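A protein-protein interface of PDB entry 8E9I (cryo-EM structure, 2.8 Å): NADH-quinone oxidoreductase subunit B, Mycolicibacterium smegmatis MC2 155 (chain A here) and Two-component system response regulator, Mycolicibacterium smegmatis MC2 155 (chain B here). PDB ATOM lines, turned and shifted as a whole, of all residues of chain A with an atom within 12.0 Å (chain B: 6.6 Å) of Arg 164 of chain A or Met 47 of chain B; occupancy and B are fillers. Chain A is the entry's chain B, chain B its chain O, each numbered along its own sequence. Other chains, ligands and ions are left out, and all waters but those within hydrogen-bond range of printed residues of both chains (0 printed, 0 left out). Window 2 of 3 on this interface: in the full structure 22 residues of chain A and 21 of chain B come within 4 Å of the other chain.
Of chain B, only Met 47 comes within 4 Å of Arg 164 of chain A.
Met 47 of chain B touches three residues of chain A.
Thr 44 of chain B touches just these residues of chain A: Glu 167 and Ala 170.
No residue of chain A comes within 4 Å of Pro 46 of chain B.
No residue of chain A comes within 4 Å of Ala 48 of chain B.
No residue of chain A comes within 4 Å of Ser 50 of chain B.
No residue of chain A comes within 4 Å of Gln 51 of chain B.
Printed residues of chain A within 4 Å of Asp 41 of chain B: Glu 167.
Of the printed residues of chain B, Ala 170 of chain A touches Ala 43 and Thr 44.
Printed residues of chain B within 4 Å of Leu 171 of chain A: Ala 43.
Ala 166 of chain A touches none of the printed residues of chain B.
The nearest printed residue of chain A that does not touch Met 47 of chain B is Glu 165 of chain A (5.7 Å).
The nearest printed residue of chain A that does not touch Asp 41 of chain B is Leu 171 of chain A (4.2 Å).
Printed residues of chain A that touch a printed residue of chain B: Ile 163, Arg 164, Glu 167, Ala 170 and Leu 171.
The backbone NH of Met 47 of chain B lies close to the side-chain hydroxyl of Thr 44 of chain B, at 3.5 Å.
The backbone carbonyl oxygen of Met 47 of chain B sits at hydrogen-bond distance from the side-chain hydroxyl of Ser 50 of chain B (2.9 Å).
Ile 163 of chain A touches Met 47 of chain B.
CE of Met 47 of chain B touches CA of Arg 164 of chain A, at 3.6 Å.
Glu 167 of chain A touches Val 42 of chain B.
Glu 167 of chain A touches Met 47 of chain B (CB to CE, 3.2 Å).
Ala 170 of chain A touches Ala 43 of chain B (CB to CB, 3.9 Å).
Ala 170 of chain A touches Thr 44 of chain B (CB to CG2, 3.6 Å).
Ala 43 of chain B touches Leu 171 of chain A.
OE1 of Glu 167 of chain A lies within hydrogen-bond range of N of Ala 43 of chain B.
The side-chain hydroxyl (OG1) of Thr 44 of chain B sits at hydrogen-bond distance from the side-chain carboxylate (OE1) of Glu 167 of chain A, at 3.4 Å.
O of Asp 41 of chain B sits close to OE2 of Glu 167 of chain A (3.2 Å).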
ATOM      1  N   PRO A 124      -0.099   3.028  21.044  1.00  0.00           N
ATOM      2  CA  PRO A 124       0.677   2.083  20.237  1.00  0.00           C
ATOM      3  C   PRO A 124       1.724   1.384  21.086  1.00  0.00           C
ATOM      4  O   PRO A 124       2.424   2.013  21.879  1.00  0.00           O
ATOM      5  CB  PRO A 124       1.316   2.971  19.164  1.00  0.00           C
ATOM      6  CG  PRO A 124       0.517   4.213  19.157  1.00  0.00           C
ATOM      7  CD  PRO A 124       0.053   4.407  20.558  1.00  0.00           C
ATOM      8  N   PRO A 154      14.091   4.270  10.533  1.00  0.00           N
ATOM      9  CA  PRO A 154      14.285   5.217   9.435  1.00  0.00           C
ATOM     10  C   PRO A 154      13.905   6.635   9.830  1.00  0.00           C
ATOM     11  O   PRO A 154      13.248   6.877  10.843  1.00  0.00           O
ATOM     12  CB  PRO A 154      13.351   4.679   8.349  1.00  0.00           C
ATOM     13  CG  PRO A 154      12.247   4.061   9.107  1.00  0.00           C
ATOM     14  CD  PRO A 154      12.856   3.489  10.359  1.00  0.00           C
ATOM     15  N   LEU A 155      14.334   7.581   8.997  1.00  0.00           N
ATOM     16  CA  LEU A 155      14.051   8.993   9.205  1.00  0.00           C
ATOM     17  C   LEU A 155      13.754   9.661   7.872  1.00  0.00           C
ATOM     18  O   LEU A 155      14.240   9.245   6.817  1.00  0.00           O
ATOM     19  CB  LEU A 155      15.219   9.720   9.884  1.00  0.00           C
ATOM     20  CG  LEU A 155      15.522   9.359  11.339  1.00  0.00           C
ATOM     21  CD1 LEU A 155      16.830   9.982  11.772  1.00  0.00           C
ATOM     22  CD2 LEU A 155      14.400   9.808  12.241  1.00  0.00           C
ATOM     23  N   GLY A 156      12.944  10.713   7.938  1.00  0.00           N
ATOM     24  CA  GLY A 156      12.652  11.499   6.755  1.00  0.00           C
ATOM     25  C   GLY A 156      12.034  10.671   5.648  1.00  0.00           C
ATOM     26  O   GLY A 156      11.121   9.865   5.864  1.00  0.00           O
ATOM     27  N   VAL A 157      12.541  10.879   4.432  1.00  0.00           N
ATOM     28  CA  VAL A 157      12.010  10.173   3.273  1.00  0.00           C
ATOM     29  C   VAL A 157      12.076   8.674   3.505  1.00  0.00           C
ATOM     30  O   VAL A 157      11.186   7.923   3.087  1.00  0.00           O
ATOM     31  CB  VAL A 157      12.775  10.586   2.003  1.00  0.00           C
ATOM     32  CG1 VAL A 157      14.250  10.231   2.126  1.00  0.00           C
ATOM     33  CG2 VAL A 157      12.162   9.924   0.781  1.00  0.00           C
ATOM     34  N   ASN A 158      13.130   8.214   4.178  1.00  0.00           N
ATOM     35  CA  ASN A 158      13.194   6.809   4.551  1.00  0.00           C
ATOM     36  C   ASN A 158      12.072   6.444   5.507  1.00  0.00           C
ATOM     37  O   ASN A 158      11.517   5.347   5.416  1.00  0.00           O
ATOM     38  CB  ASN A 158      14.548   6.489   5.175  1.00  0.00           C
ATOM     39  CG  ASN A 158      15.702   6.796   4.247  1.00  0.00           C
ATOM     40  OD1 ASN A 158      15.612   6.587   3.041  1.00  0.00           O
ATOM     41  ND2 ASN A 158      16.797   7.290   4.808  1.00  0.00           N
ATOM     42  N   ARG A 159      11.722   7.343   6.428  1.00  0.00           N
ATOM     43  CA  ARG A 159      10.606   7.063   7.324  1.00  0.00           C
ATOM     44  C   ARG A 159       9.314   6.889   6.542  1.00  0.00           C
ATOM     45  O   ARG A 159       8.535   5.968   6.810  1.00  0.00           O
ATOM     46  CB  ARG A 159      10.456   8.183   8.352  1.00  0.00           C
ATOM     47  N   GLU A 160       9.067   7.766   5.571  1.00  0.00           N
ATOM     48  CA  GLU A 160       7.849   7.656   4.774  1.00  0.00           C
ATOM     49  C   GLU A 160       7.842   6.364   3.959  1.00  0.00           C
ATOM     50  O   GLU A 160       6.820   5.671   3.873  1.00  0.00           O
ATOM     51  CB  GLU A 160       7.709   8.873   3.860  1.00  0.00           C
ATOM     52  N   GLU A 161       8.981   6.023   3.354  1.00  0.00           N
ATOM     53  CA  GLU A 161       9.058   4.788   2.584  1.00  0.00           C
ATOM     54  C   GLU A 161       8.813   3.576   3.471  1.00  0.00           C
ATOM     55  O   GLU A 161       8.127   2.631   3.069  1.00  0.00           O
ATOM     56  CB  GLU A 161      10.420   4.680   1.901  1.00  0.00           C
ATOM     57  N   ALA A 162       9.378   3.579   4.676  1.00  0.00           N
ATOM     58  CA  ALA A 162       9.158   2.475   5.597  1.00  0.00           C
ATOM     59  C   ALA A 162       7.700   2.387   6.016  1.00  0.00           C
ATOM     60  O   ALA A 162       7.150   1.289   6.133  1.00  0.00           O
ATOM     61  CB  ALA A 162      10.053   2.628   6.822  1.00  0.00           C
ATOM     62  N   ILE A 163       7.055   3.525   6.266  1.00  0.00           N
ATOM     63  CA  ILE A 163       5.641   3.483   6.625  1.00  0.00           C
ATOM     64  C   ILE A 163       4.835   2.881   5.485  1.00  0.00           C
ATOM     65  O   ILE A 163       3.961   2.037   5.705  1.00  0.00           O
ATOM     66  CB  ILE A 163       5.132   4.884   7.010  1.00  0.00           C
ATOM     67  CG1 ILE A 163       5.530   5.200   8.453  1.00  0.00           C
ATOM     68  CG2 ILE A 163       3.625   4.967   6.854  1.00  0.00           C
ATOM     69  CD1 ILE A 163       5.348   6.642   8.841  1.00  0.00           C
ATOM     70  N   ARG A 164       5.128   3.287   4.249  1.00  0.00           N
ATOM     71  CA  ARG A 164       4.402   2.735   3.110  1.00  0.00           C
ATOM     72  C   ARG A 164       4.632   1.233   2.979  1.00  0.00           C
ATOM     73  O   ARG A 164       3.684   0.467   2.763  1.00  0.00           O
ATOM     74  CB  ARG A 164       4.813   3.457   1.828  1.00  0.00           C
ATOM     75  N   GLU A 165       5.881   0.791   3.110  1.00  0.00           N
ATOM     76  CA  GLU A 165       6.172  -0.632   2.978  1.00  0.00           C
ATOM     77  C   GLU A 165       5.489  -1.434   4.078  1.00  0.00           C
ATOM     78  O   GLU A 165       4.897  -2.489   3.817  1.00  0.00           O
ATOM     79  CB  GLU A 165       7.682  -0.862   3.003  1.00  0.00           C
ATOM     80  N   ALA A 166       5.564  -0.950   5.319  1.00  0.00           N
ATOM     81  CA  ALA A 166       4.931  -1.657   6.423  1.00  0.00           C
ATOM     82  C   ALA A 166       3.427  -1.709   6.237  1.00  0.00           C
ATOM     83  O   ALA A 166       2.796  -2.730   6.520  1.00  0.00           O
ATOM     84  CB  ALA A 166       5.282  -0.989   7.750  1.00  0.00           C
ATOM     85  N   GLU A 167       2.831  -0.616   5.767  1.00  0.00           N
ATOM     86  CA  GLU A 167       1.397  -0.617   5.527  1.00  0.00           C
ATOM     87  C   GLU A 167       1.025  -1.649   4.475  1.00  0.00           C
ATOM     88  O   GLU A 167       0.084  -2.429   4.659  1.00  0.00           O
ATOM     89  CB  GLU A 167       0.940   0.778   5.101  1.00  0.00           C
ATOM     90  CG  GLU A 167      -0.352   0.796   4.308  1.00  0.00           C
ATOM     91  CD  GLU A 167      -1.515   0.257   5.103  1.00  0.00           C
ATOM     92  OE1 GLU A 167      -1.301  -0.195   6.245  1.00  0.00           O
ATOM     93  OE2 GLU A 167      -2.649   0.282   4.585  1.00  0.00           O
ATOM     94  N   GLN A 168       1.754  -1.671   3.359  1.00  0.00           N
ATOM     95  CA  GLN A 168       1.439  -2.631   2.309  1.00  0.00           C
ATOM     96  C   GLN A 168       1.568  -4.056   2.825  1.00  0.00           C
ATOM     97  O   GLN A 168       0.707  -4.902   2.565  1.00  0.00           O
ATOM     98  CB  GLN A 168       2.351  -2.411   1.101  1.00  0.00           C
ATOM     99  N   ALA A 169       2.636  -4.337   3.574  1.00  0.00           N
ATOM    100  CA  ALA A 169       2.829  -5.682   4.102  1.00  0.00           C
ATOM    101  C   ALA A 169       1.714  -6.053   5.067  1.00  0.00           C
ATOM    102  O   ALA A 169       1.208  -7.180   5.050  1.00  0.00           O
ATOM    103  CB  ALA A 169       4.189  -5.784   4.789  1.00  0.00           C
ATOM    104  N   ALA A 170       1.311  -5.109   5.920  1.00  0.00           N
ATOM    105  CA  ALA A 170       0.327  -5.408   6.952  1.00  0.00           C
ATOM    106  C   ALA A 170      -1.040  -5.715   6.362  1.00  0.00           C
ATOM    107  O   ALA A 170      -1.828  -6.441   6.974  1.00  0.00           O
ATOM    108  CB  ALA A 170       0.223  -4.238   7.927  1.00  0.00           C
ATOM    109  N   LEU A 171      -1.344  -5.167   5.189  1.00  0.00           N
ATOM    110  CA  LEU A 171      -2.669  -5.359   4.614  1.00  0.00           C
ATOM    111  C   LEU A 171      -2.901  -6.805   4.201  1.00  0.00           C
ATOM    112  O   LEU A 171      -4.047  -7.211   3.984  1.00  0.00           O
ATOM    113  CB  LEU A 171      -2.850  -4.432   3.416  1.00  0.00           C
ATOM    114  CG  LEU A 171      -3.195  -2.984   3.765  1.00  0.00           C
ATOM    115  CD1 LEU A 171      -2.922  -2.075   2.580  1.00  0.00           C
ATOM    116  CD2 LEU A 171      -4.633  -2.868   4.209  1.00  0.00           C
ATOM    117  N   ALA A 172      -1.838  -7.599   4.093  1.00  0.00           N
ATOM    118  CA  ALA A 172      -1.943  -8.940   3.541  1.00  0.00           C
ATOM    119  C   ALA A 172      -2.004 -10.039   4.593  1.00  0.00           C
ATOM    120  O   ALA A 172      -2.566 -11.104   4.314  1.00  0.00           O
ATOM    121  CB  ALA A 172      -0.759  -9.212   2.611  1.00  0.00           C
ATOM    122  N   VAL A 173      -1.456  -9.816   5.782  1.00  0.00           N
ATOM    123  CA  VAL A 173      -1.391 -10.895   6.777  1.00  0.00           C
ATOM    124  C   VAL A 173      -2.803 -11.360   7.108  1.00  0.00           C
ATOM    125  O   VAL A 173      -3.650 -10.528   7.477  1.00  0.00           O
ATOM    126  CB  VAL A 173      -0.663 -10.420   8.037  1.00  0.00           C
ATOM    127  CG1 VAL A 173       0.774 -10.038   7.717  1.00  0.00           C
ATOM    128  CG2 VAL A 173      -1.405  -9.253   8.684  1.00  0.00           C
ATOM    129  N   LEU B  10     -11.953   6.467   5.743  1.00  0.00           N
ATOM    130  CA  LEU B  10     -10.784   5.733   6.197  1.00  0.00           C
ATOM    131  C   LEU B  10     -11.233   4.625   7.139  1.00  0.00           C
ATOM    132  O   LEU B  10     -11.711   4.897   8.244  1.00  0.00           O
ATOM    133  CB  LEU B  10      -9.800   6.665   6.894  1.00  0.00           C
ATOM    134  CG  LEU B  10      -8.498   6.003   7.339  1.00  0.00           C
ATOM    135  CD1 LEU B  10      -7.621   5.679   6.145  1.00  0.00           C
ATOM    136  CD2 LEU B  10      -7.767   6.900   8.309  1.00  0.00           C
ATOM    137  N   ASP B  41      -8.183   1.955   2.764  1.00  0.00           N
ATOM    138  CA  ASP B  41      -8.007   0.997   3.842  1.00  0.00           C
ATOM    139  C   ASP B  41      -6.588   1.079   4.379  1.00  0.00           C
ATOM    140  O   ASP B  41      -5.620   1.142   3.618  1.00  0.00           O
ATOM    141  CB  ASP B  41      -8.294  -0.426   3.364  1.00  0.00           C
ATOM    142  CG  ASP B  41      -9.771  -0.732   3.314  1.00  0.00           C
ATOM    143  OD1 ASP B  41     -10.577   0.148   3.682  1.00  0.00           O
ATOM    144  OD2 ASP B  41     -10.134  -1.852   2.897  1.00  0.00           O
ATOM    145  N   VAL B  42      -6.472   1.073   5.704  1.00  0.00           N
ATOM    146  CA  VAL B  42      -5.188   1.173   6.377  1.00  0.00           C
ATOM    147  C   VAL B  42      -5.137   0.122   7.475  1.00  0.00           C
ATOM    148  O   VAL B  42      -6.119  -0.133   8.172  1.00  0.00           O
ATOM    149  CB  VAL B  42      -4.948   2.581   6.954  1.00  0.00           C
ATOM    150  CG1 VAL B  42      -4.731   3.570   5.832  1.00  0.00           C
ATOM    151  CG2 VAL B  42      -6.118   3.009   7.810  1.00  0.00           C
ATOM    152  N   ALA B  43      -3.961  -0.496   7.620  1.00  0.00           N
ATOM    153  CA  ALA B  43      -3.800  -1.550   8.617  1.00  0.00           C
ATOM    154  C   ALA B  43      -2.720  -1.228   9.643  1.00  0.00           C
ATOM    155  O   ALA B  43      -2.281  -2.137  10.357  1.00  0.00           O
ATOM    156  CB  ALA B  43      -3.463  -2.878   7.935  1.00  0.00           C
ATOM    157  N   THR B  44      -2.277   0.024   9.741  1.00  0.00           N
ATOM    158  CA  THR B  44      -1.240   0.398  10.700  1.00  0.00           C
ATOM    159  C   THR B  44      -1.595   1.785  11.225  1.00  0.00           C
ATOM    160  O   THR B  44      -2.114   2.619  10.479  1.00  0.00           O
ATOM    161  CB  THR B  44       0.140   0.385  10.063  1.00  0.00           C
ATOM    162  OG1 THR B  44       0.169   1.296   8.958  1.00  0.00           O
ATOM    163  CG2 THR B  44       0.484  -1.002   9.569  1.00  0.00           C
ATOM    164  N   ALA B  45      -1.326   2.017  12.505  1.00  0.00           N
ATOM    165  CA  ALA B  45      -1.606   3.311  13.106  1.00  0.00           C
ATOM    166  C   ALA B  45      -0.836   4.422  12.404  1.00  0.00           C
ATOM    167  O   ALA B  45      -1.423   5.465  12.104  1.00  0.00           O
ATOM    168  CB  ALA B  45      -1.280   3.297  14.599  1.00  0.00           C
ATOM    169  N   PRO B  46       0.467   4.268  12.141  1.00  0.00           N
ATOM    170  CA  PRO B  46       1.188   5.363  11.468  1.00  0.00           C
ATOM    171  C   PRO B  46       0.582   5.744  10.134  1.00  0.00           C
ATOM    172  O   PRO B  46       0.460   6.934   9.825  1.00  0.00           O
ATOM    173  CB  PRO B  46       2.603   4.795  11.303  1.00  0.00           C
ATOM    174  CG  PRO B  46       2.718   3.766  12.353  1.00  0.00           C
ATOM    175  CD  PRO B  46       1.364   3.147  12.454  1.00  0.00           C
ATOM    176  N   MET B  47       0.171   4.758   9.336  1.00  0.00           N
ATOM    177  CA  MET B  47      -0.445   5.061   8.052  1.00  0.00           C
ATOM    178  C   MET B  47      -1.802   5.717   8.234  1.00  0.00           C
ATOM    179  O   MET B  47      -2.156   6.644   7.501  1.00  0.00           O
ATOM    180  CB  MET B  47      -0.581   3.792   7.219  1.00  0.00           C
ATOM    181  CG  MET B  47      -1.110   4.049   5.826  1.00  0.00           C
ATOM    182  SD  MET B  47      -0.017   5.064   4.831  1.00  0.00           S
ATOM    183  CE  MET B  47       1.306   3.913   4.503  1.00  0.00           C
ATOM    184  N   ALA B  48      -2.592   5.231   9.187  1.00  0.00           N
ATOM    185  CA  ALA B  48      -3.887   5.847   9.439  1.00  0.00           C
ATOM    186  C   ALA B  48      -3.709   7.307   9.818  1.00  0.00           C
ATOM    187  O   ALA B  48      -4.415   8.190   9.317  1.00  0.00           O
ATOM    188  CB  ALA B  48      -4.613   5.086  10.545  1.00  0.00           C
ATOM    189  N   ILE B  49      -2.739   7.579  10.688  1.00  0.00           N
ATOM    190  CA  ILE B  49      -2.477   8.946  11.115  1.00  0.00           C
ATOM    191  C   ILE B  49      -2.035   9.792   9.929  1.00  0.00           C
ATOM    192  O   ILE B  49      -2.494  10.922   9.750  1.00  0.00           O
ATOM    193  CB  ILE B  49      -1.426   8.959  12.239  1.00  0.00           C
ATOM    194  CG1 ILE B  49      -1.983   8.302  13.505  1.00  0.00           C
ATOM    195  CG2 ILE B  49      -0.984  10.377  12.536  1.00  0.00           C
ATOM    196  CD1 ILE B  49      -3.139   9.045  14.141  1.00  0.00           C
ATOM    197  N   SER B  50      -1.131   9.262   9.103  1.00  0.00           N
ATOM    198  CA  SER B  50      -0.649  10.038   7.966  1.00  0.00           C
ATOM    199  C   SER B  50      -1.762  10.324   6.966  1.00  0.00           C
ATOM    200  O   SER B  50      -1.842  11.433   6.431  1.00  0.00           O
ATOM    201  CB  SER B  50       0.506   9.310   7.283  1.00  0.00           C
ATOM    202  OG  SER B  50       0.043   8.193   6.550  1.00  0.00           O
ATOM    203  N   GLN B  51      -2.621   9.342   6.696  1.00  0.00           N
ATOM    204  CA  GLN B  51      -3.756   9.572   5.810  1.00  0.00           C
ATOM    205  C   GLN B  51      -4.686  10.633   6.379  1.00  0.00           C
ATOM    206  O   GLN B  51      -5.147  11.517   5.651  1.00  0.00           O
ATOM    207  CB  GLN B  51      -4.519   8.268   5.585  1.00  0.00           C
ATOM    208  CG  GLN B  51      -3.796   7.246   4.729  1.00  0.00           C
ATOM    209  CD  GLN B  51      -3.683   7.670   3.285  1.00  0.00           C
ATOM    210  OE1 GLN B  51      -4.436   8.521   2.818  1.00  0.00           O
ATOM    211  NE2 GLN B  51      -2.757   7.059   2.560  1.00  0.00           N
ATOM    212  N   MET B  52      -4.969  10.567   7.678  1.00  0.00           N
ATOM    213  CA  MET B  52      -5.763  11.617   8.300  1.00  0.00           C
ATOM    214  C   MET B  52      -5.090  12.972   8.134  1.00  0.00           C
ATOM    215  O   MET B  52      -5.748  13.964   7.805  1.00  0.00           O
ATOM    216  CB  MET B  52      -5.963  11.301   9.779  1.00  0.00           C
ATOM    217  CG  MET B  52      -6.796  10.061  10.043  1.00  0.00           C
ATOM    218  SD  MET B  52      -8.464  10.199   9.389  1.00  0.00           S
ATOM    219  CE  MET B  52      -9.117  11.439  10.498  1.00  0.00           C
